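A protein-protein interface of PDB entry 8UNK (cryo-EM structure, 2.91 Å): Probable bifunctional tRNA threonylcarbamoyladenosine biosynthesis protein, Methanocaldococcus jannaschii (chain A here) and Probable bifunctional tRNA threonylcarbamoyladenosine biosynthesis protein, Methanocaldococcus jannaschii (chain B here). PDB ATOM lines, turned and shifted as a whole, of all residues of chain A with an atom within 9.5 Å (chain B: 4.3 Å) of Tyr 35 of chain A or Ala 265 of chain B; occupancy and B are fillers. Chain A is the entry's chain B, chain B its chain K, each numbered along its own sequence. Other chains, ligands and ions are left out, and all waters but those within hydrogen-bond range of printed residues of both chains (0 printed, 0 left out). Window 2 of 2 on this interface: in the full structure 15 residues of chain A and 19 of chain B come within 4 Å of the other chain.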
ATOM      1  N   VAL A  31       4.863  12.926  -1.204  1.00  0.00           N
ATOM      2  CA  VAL A  31       5.827  12.012  -0.606  1.00  0.00           C
ATOM      3  C   VAL A  31       6.178  10.901  -1.593  1.00  0.00           C
ATOM      4  O   VAL A  31       5.413  10.569  -2.505  1.00  0.00           O
ATOM      5  CB  VAL A  31       5.291  11.426   0.710  1.00  0.00           C
ATOM      6  CG1 VAL A  31       5.048  12.533   1.723  1.00  0.00           C
ATOM      7  CG2 VAL A  31       4.016  10.631   0.463  1.00  0.00           C
ATOM      8  N   LYS A  32       7.362  10.326  -1.399  1.00  0.00           N
ATOM      9  CA  LYS A  32       7.862   9.255  -2.257  1.00  0.00           C
ATOM     10  C   LYS A  32       7.363   7.925  -1.711  1.00  0.00           C
ATOM     11  O   LYS A  32       7.993   7.321  -0.840  1.00  0.00           O
ATOM     12  CB  LYS A  32       9.384   9.287  -2.322  1.00  0.00           C
ATOM     13  N   LYS A  33       6.223   7.462  -2.224  1.00  0.00           N
ATOM     14  CA  LYS A  33       5.665   6.187  -1.795  1.00  0.00           C
ATOM     15  C   LYS A  33       6.665   5.070  -2.064  1.00  0.00           C
ATOM     16  O   LYS A  33       7.092   4.869  -3.206  1.00  0.00           O
ATOM     17  CB  LYS A  33       4.339   5.911  -2.505  1.00  0.00           C
ATOM     18  N   GLY A  34       7.041   4.341  -1.014  1.00  0.00           N
ATOM     19  CA  GLY A  34       8.089   3.346  -1.149  1.00  0.00           C
ATOM     20  C   GLY A  34       7.723   2.202  -2.074  1.00  0.00           C
ATOM     21  O   GLY A  34       8.590   1.651  -2.757  1.00  0.00           O
ATOM     22  N   TYR A  35       6.443   1.828  -2.113  1.00  0.00           N
ATOM     23  CA  TYR A  35       6.050   0.635  -2.853  1.00  0.00           C
ATOM     24  C   TYR A  35       6.342   0.748  -4.344  1.00  0.00           C
ATOM     25  O   TYR A  35       6.406  -0.279  -5.027  1.00  0.00           O
ATOM     26  CB  TYR A  35       4.563   0.342  -2.627  1.00  0.00           C
ATOM     27  CG  TYR A  35       3.596   1.347  -3.223  1.00  0.00           C
ATOM     28  CD1 TYR A  35       3.411   1.440  -4.599  1.00  0.00           C
ATOM     29  CD2 TYR A  35       2.852   2.189  -2.408  1.00  0.00           C
ATOM     30  CE1 TYR A  35       2.528   2.348  -5.142  1.00  0.00           C
ATOM     31  CE2 TYR A  35       1.963   3.098  -2.944  1.00  0.00           C
ATOM     32  CZ  TYR A  35       1.804   3.174  -4.312  1.00  0.00           C
ATOM     33  OH  TYR A  35       0.922   4.079  -4.853  1.00  0.00           O
ATOM     34  N   ARG A  36       6.522   1.955  -4.864  1.00  0.00           N
ATOM     35  CA  ARG A  36       6.700   2.159  -6.293  1.00  0.00           C
ATOM     36  C   ARG A  36       8.164   2.421  -6.624  1.00  0.00           C
ATOM     37  O   ARG A  36       8.993   2.694  -5.753  1.00  0.00           O
ATOM     38  CB  ARG A  36       5.823   3.316  -6.785  1.00  0.00           C
ATOM     39  CG  ARG A  36       5.830   4.549  -5.900  1.00  0.00           C
ATOM     40  CD  ARG A  36       5.152   5.712  -6.603  1.00  0.00           C
ATOM     41  NE  ARG A  36       4.216   6.410  -5.732  1.00  0.00           N
ATOM     42  CZ  ARG A  36       3.258   7.220  -6.160  1.00  0.00           C
ATOM     43  NH1 ARG A  36       3.090   7.474  -7.448  1.00  0.00           N
ATOM     44  NH2 ARG A  36       2.447   7.792  -5.273  1.00  0.00           N
ATOM     45  N   ASP A  37       8.473   2.329  -7.915  1.00  0.00           N
ATOM     46  CA  ASP A  37       9.837   2.536  -8.376  1.00  0.00           C
ATOM     47  C   ASP A  37      10.288   3.956  -8.066  1.00  0.00           C
ATOM     48  O   ASP A  37       9.575   4.921  -8.350  1.00  0.00           O
ATOM     49  CB  ASP A  37       9.924   2.264  -9.876  1.00  0.00           C
ATOM     50  CG  ASP A  37      11.349   2.212 -10.377  1.00  0.00           C
ATOM     51  OD1 ASP A  37      12.270   2.539  -9.603  1.00  0.00           O
ATOM     52  OD2 ASP A  37      11.549   1.836 -11.548  1.00  0.00           O
ATOM     53  N   GLU A  38      11.488   4.081  -7.497  1.00  0.00           N
ATOM     54  CA  GLU A  38      11.977   5.395  -7.091  1.00  0.00           C
ATOM     55  C   GLU A  38      12.099   6.333  -8.284  1.00  0.00           C
ATOM     56  O   GLU A  38      11.731   7.510  -8.196  1.00  0.00           O
ATOM     57  CB  GLU A  38      13.324   5.255  -6.381  1.00  0.00           C
ATOM     58  N   LEU A  40      10.502   6.370 -11.421  1.00  0.00           N
ATOM     59  CA  LEU A  40       9.192   6.837 -11.856  1.00  0.00           C
ATOM     60  C   LEU A  40       8.430   7.498 -10.716  1.00  0.00           C
ATOM     61  O   LEU A  40       7.609   8.383 -10.962  1.00  0.00           O
ATOM     62  CB  LEU A  40       8.383   5.677 -12.438  1.00  0.00           C
ATOM     63  CG  LEU A  40       6.956   5.990 -12.897  1.00  0.00           C
ATOM     64  CD1 LEU A  40       6.982   6.634 -14.271  1.00  0.00           C
ATOM     65  CD2 LEU A  40       6.096   4.736 -12.907  1.00  0.00           C
ATOM     66  N   ASP A  41       8.681   7.095  -9.471  1.00  0.00           N
ATOM     67  CA  ASP A  41       8.035   7.770  -8.349  1.00  0.00           C
ATOM     68  C   ASP A  41       8.396   9.248  -8.327  1.00  0.00           C
ATOM     69  O   ASP A  41       7.517  10.116  -8.271  1.00  0.00           O
ATOM     70  CB  ASP A  41       8.432   7.104  -7.032  1.00  0.00           C
ATOM     71  CG  ASP A  41       7.922   7.858  -5.826  1.00  0.00           C
ATOM     72  OD1 ASP A  41       6.760   8.310  -5.855  1.00  0.00           O
ATOM     73  OD2 ASP A  41       8.680   7.996  -4.846  1.00  0.00           O
ATOM     74  N   ILE A  44       6.904  11.095 -11.431  1.00  0.00           N
ATOM     75  CA  ILE A  44       5.479  11.381 -11.333  1.00  0.00           C
ATOM     76  C   ILE A  44       5.217  12.441 -10.277  1.00  0.00           C
ATOM     77  O   ILE A  44       4.348  13.299 -10.454  1.00  0.00           O
ATOM     78  CB  ILE A  44       4.699  10.084 -11.052  1.00  0.00           C
ATOM     79  CG1 ILE A  44       4.368   9.387 -12.374  1.00  0.00           C
ATOM     80  CG2 ILE A  44       3.432  10.371 -10.249  1.00  0.00           C
ATOM     81  CD1 ILE A  44       3.763   8.020 -12.213  1.00  0.00           C
ATOM     82  N   ARG A  48       3.367  15.858 -11.289  1.00  0.00           N
ATOM     83  CA  ARG A  48       2.106  16.207 -10.654  1.00  0.00           C
ATOM     84  C   ARG A  48       2.215  17.525  -9.904  1.00  0.00           C
ATOM     85  O   ARG A  48       1.276  18.324  -9.918  1.00  0.00           O
ATOM     86  CB  ARG A  48       1.668  15.086  -9.717  1.00  0.00           C
ATOM     87  CG  ARG A  48       0.960  13.959 -10.438  1.00  0.00           C
ATOM     88  CD  ARG A  48       0.508  12.881  -9.482  1.00  0.00           C
ATOM     89  NE  ARG A  48      -0.271  11.855 -10.161  1.00  0.00           N
ATOM     90  CZ  ARG A  48      -0.663  10.720  -9.600  1.00  0.00           C
ATOM     91  NH1 ARG A  48      -0.367  10.430  -8.345  1.00  0.00           N
ATOM     92  NH2 ARG A  48      -1.375   9.858 -10.316  1.00  0.00           N
ATOM     93  N   SER B 229       1.309   0.073 -10.311  1.00  0.00           N
ATOM     94  CA  SER B 229       1.352   1.252  -9.458  1.00  0.00           C
ATOM     95  C   SER B 229      -0.010   1.928  -9.382  1.00  0.00           C
ATOM     96  O   SER B 229      -0.435   2.349  -8.303  1.00  0.00           O
ATOM     97  CB  SER B 229       2.412   2.219  -9.979  1.00  0.00           C
ATOM     98  OG  SER B 229       2.430   2.223 -11.395  1.00  0.00           O
ATOM     99  N   THR B 232      -2.198  -0.260  -7.285  1.00  0.00           N
ATOM    100  CA  THR B 232      -1.815  -0.073  -5.894  1.00  0.00           C
ATOM    101  C   THR B 232      -2.361   1.238  -5.347  1.00  0.00           C
ATOM    102  O   THR B 232      -2.827   1.300  -4.205  1.00  0.00           O
ATOM    103  CB  THR B 232      -0.290  -0.104  -5.790  1.00  0.00           C
ATOM    104  OG1 THR B 232       0.234  -1.041  -6.738  1.00  0.00           O
ATOM    105  CG2 THR B 232       0.161  -0.501  -4.403  1.00  0.00           C
ATOM    106  N   GLU B 233      -2.319   2.299  -6.151  1.00  0.00           N
ATOM    107  CA  GLU B 233      -2.776   3.596  -5.668  1.00  0.00           C
ATOM    108  C   GLU B 233      -4.286   3.614  -5.473  1.00  0.00           C
ATOM    109  O   GLU B 233      -4.778   4.162  -4.482  1.00  0.00           O
ATOM    110  CB  GLU B 233      -2.343   4.698  -6.633  1.00  0.00           C
ATOM    111  CG  GLU B 233      -2.051   6.022  -5.945  1.00  0.00           C
ATOM    112  CD  GLU B 233      -2.406   7.218  -6.801  1.00  0.00           C
ATOM    113  OE1 GLU B 233      -2.954   8.198  -6.254  1.00  0.00           O
ATOM    114  OE2 GLU B 233      -2.133   7.178  -8.018  1.00  0.00           O
ATOM    115  N   GLU B 261       4.461  -8.104  -4.770  1.00  0.00           N
ATOM    116  CA  GLU B 261       5.388  -7.377  -3.913  1.00  0.00           C
ATOM    117  C   GLU B 261       5.069  -5.888  -3.871  1.00  0.00           C
ATOM    118  O   GLU B 261       5.241  -5.260  -2.822  1.00  0.00           O
ATOM    119  CB  GLU B 261       6.837  -7.609  -4.350  1.00  0.00           C
ATOM    120  CG  GLU B 261       7.169  -7.192  -5.763  1.00  0.00           C
ATOM    121  CD  GLU B 261       8.514  -7.715  -6.223  1.00  0.00           C
ATOM    122  OE1 GLU B 261       8.605  -8.916  -6.553  1.00  0.00           O
ATOM    123  OE2 GLU B 261       9.482  -6.927  -6.255  1.00  0.00           O
ATOM    124  N   MET B 262       4.593  -5.294  -4.972  1.00  0.00           N
ATOM    125  CA  MET B 262       4.173  -3.896  -4.877  1.00  0.00           C
ATOM    126  C   MET B 262       3.009  -3.753  -3.904  1.00  0.00           C
ATOM    127  O   MET B 262       2.990  -2.839  -3.069  1.00  0.00           O
ATOM    128  CB  MET B 262       3.789  -3.313  -6.241  1.00  0.00           C
ATOM    129  CG  MET B 262       4.481  -3.910  -7.443  1.00  0.00           C
ATOM    130  SD  MET B 262       4.367  -2.938  -8.960  1.00  0.00           S
ATOM    131  CE  MET B 262       4.803  -1.294  -8.402  1.00  0.00           C
ATOM    132  N   LEU B 263       2.030  -4.656  -3.990  1.00  0.00           N
ATOM    133  CA  LEU B 263       0.898  -4.597  -3.071  1.00  0.00           C
ATOM    134  C   LEU B 263       1.341  -4.834  -1.633  1.00  0.00           C
ATOM    135  O   LEU B 263       0.836  -4.189  -0.709  1.00  0.00           O
ATOM    136  CB  LEU B 263      -0.165  -5.617  -3.473  1.00  0.00           C
ATOM    137  CG  LEU B 263      -1.280  -5.164  -4.420  1.00  0.00           C
ATOM    138  CD1 LEU B 263      -2.004  -3.941  -3.880  1.00  0.00           C
ATOM    139  CD2 LEU B 263      -0.725  -4.891  -5.803  1.00  0.00           C
ATOM    140  N   LYS B 264       2.275  -5.763  -1.424  1.00  0.00           N
ATOM    141  CA  LYS B 264       2.768  -6.028  -0.078  1.00  0.00           C
ATOM    142  C   LYS B 264       3.494  -4.817   0.487  1.00  0.00           C
ATOM    143  O   LYS B 264       3.316  -4.468   1.659  1.00  0.00           O
ATOM    144  CB  LYS B 264       3.690  -7.247  -0.089  1.00  0.00           C
ATOM    145  N   ALA B 265       4.325  -4.166  -0.329  1.00  0.00           N
ATOM    146  CA  ALA B 265       5.004  -2.958   0.120  1.00  0.00           C
ATOM    147  C   ALA B 265       3.996  -1.879   0.484  1.00  0.00           C
ATOM    148  O   ALA B 265       4.110  -1.236   1.536  1.00  0.00           O
ATOM    149  CB  ALA B 265       5.956  -2.463  -0.969  1.00  0.00           C
ATOM    150  N   MET B 266       2.989  -1.676  -0.368  1.00  0.00           N
ATOM    151  CA  MET B 266       1.951  -0.702  -0.049  1.00  0.00           C
ATOM    152  C   MET B 266       1.307  -1.027   1.289  1.00  0.00           C
ATOM    153  O   MET B 266       1.227  -0.175   2.180  1.00  0.00           O
ATOM    154  CB  MET B 266       0.891  -0.675  -1.152  1.00  0.00           C
ATOM    155  CG  MET B 266      -0.380   0.102  -0.786  1.00  0.00           C
ATOM    156  SD  MET B 266      -1.772  -0.223  -1.880  1.00  0.00           S
ATOM    157  CE  MET B 266      -2.823  -1.201  -0.816  1.00  0.00           C
ATOM    158  N   CYS B 267       0.853  -2.271   1.450  1.00  0.00           N
ATOM    159  CA  CYS B 267       0.091  -2.633   2.636  1.00  0.00           C
ATOM    160  C   CYS B 267       0.940  -2.515   3.895  1.00  0.00           C
ATOM    161  O   CYS B 267       0.448  -2.079   4.943  1.00  0.00           O
ATOM    162  CB  CYS B 267      -0.465  -4.047   2.478  1.00  0.00           C
ATOM    163  SG  CYS B 267      -1.838  -4.150   1.315  1.00  0.00           S
ATOM    164  N   GLU B 268       2.215  -2.900   3.815  1.00  0.00           N
ATOM    165  CA  GLU B 268       3.115  -2.697   4.944  1.00  0.00           C
ATOM    166  C   GLU B 268       3.260  -1.215   5.257  1.00  0.00           C
ATOM    167  O   GLU B 268       3.283  -0.820   6.428  1.00  0.00           O
ATOM    168  CB  GLU B 268       4.478  -3.320   4.645  1.00  0.00           C
ATOM    169  CG  GLU B 268       4.462  -4.840   4.592  1.00  0.00           C
ATOM    170  CD  GLU B 268       5.682  -5.417   3.902  1.00  0.00           C
ATOM    171  OE1 GLU B 268       6.323  -4.691   3.113  1.00  0.00           O
ATOM    172  OE2 GLU B 268       6.001  -6.598   4.149  1.00  0.00           O
ATOM    173  N   GLY B 269       3.359  -0.379   4.222  1.00  0.00           N
ATOM    174  CA  GLY B 269       3.401   1.054   4.449  1.00  0.00           C
ATOM    175  C   GLY B 269       2.147   1.578   5.119  1.00  0.00           C
ATOM    176  O   GLY B 269       2.205   2.547   5.880  1.00  0.00           O
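OE2 of Glu 233 of chain B is in salt-bridge range of NH2 of Arg 48 of chain A (3.6 Å).
CG2 of Thr 232 of chain B touches CE1 of Tyr 35 of chain A, 3.8 Å away.
Tyr 35 of chain A touches Glu 233 of chain B (OH to CG, 3.7 Å).
Met 262 of chain B touches Tyr 35 of chain A (O to CB, 3.6 Å).
Tyr 35 of chain A touches Ala 265 of chain B.
Met 266 of chain B touches Tyr 35 of chain A (N to CB, 3.4 Å).
Tyr 35 of chain A touches five residues of chain B.
Of the printed residues of chain A, Ala 265 of chain B touches Tyr 35 (3.5 Å).
Of chain A, only Tyr 35 comes within 4 Å of Met 262 of chain B.
No residue of chain A comes within 4 Å of Lys 264 of chain B.
Glu 268 of chain B touches none of the printed residues of chain A.
Of the printed residues of chain A, Thr 232 of chain B touches Tyr 35 (3.8 Å).
Of the printed residues of chain A, Met 266 of chain B touches Tyr 35 (3.4 Å).
Of the printed residues of chain B, Arg 48 of chain A touches Glu 233.
Of the printed residues of chain A, Glu 233 of chain B touches Tyr 35 and Arg 48.
Asp 37 of chain A touches none of the printed residues of chain B.
The nearest residue of chain A that does not touch Ala 265 of chain B is Gly 34 of chain A (5.1 Å).
The nearest printed residue of chain A that does not touch Glu 233 of chain B is Arg 36 of chain A (4.9 Å).
Printed residues of chain A that touch a printed residue of chain B: Tyr 35 and Arg 48.
Hydrophobic or aromatic side chains of chain A that line the printed part of chain B: Tyr 35.
Of the 12 printed residues of chain B, 5 touch a printed residue of chain A.
Hydrophobic or aromatic side chains of chain B that line the printed part of chain A: Met 262, Ala 265 and Met 266.
Among the printed residues, 6 pairs touch across the chains.
Among the printed residues, Asp or Glu carboxylates within 4 Å of a Lys or Arg side-chain nitrogen of the other chain: Arg 48 of chain A with Glu 233 of chain B (3.6 Å).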
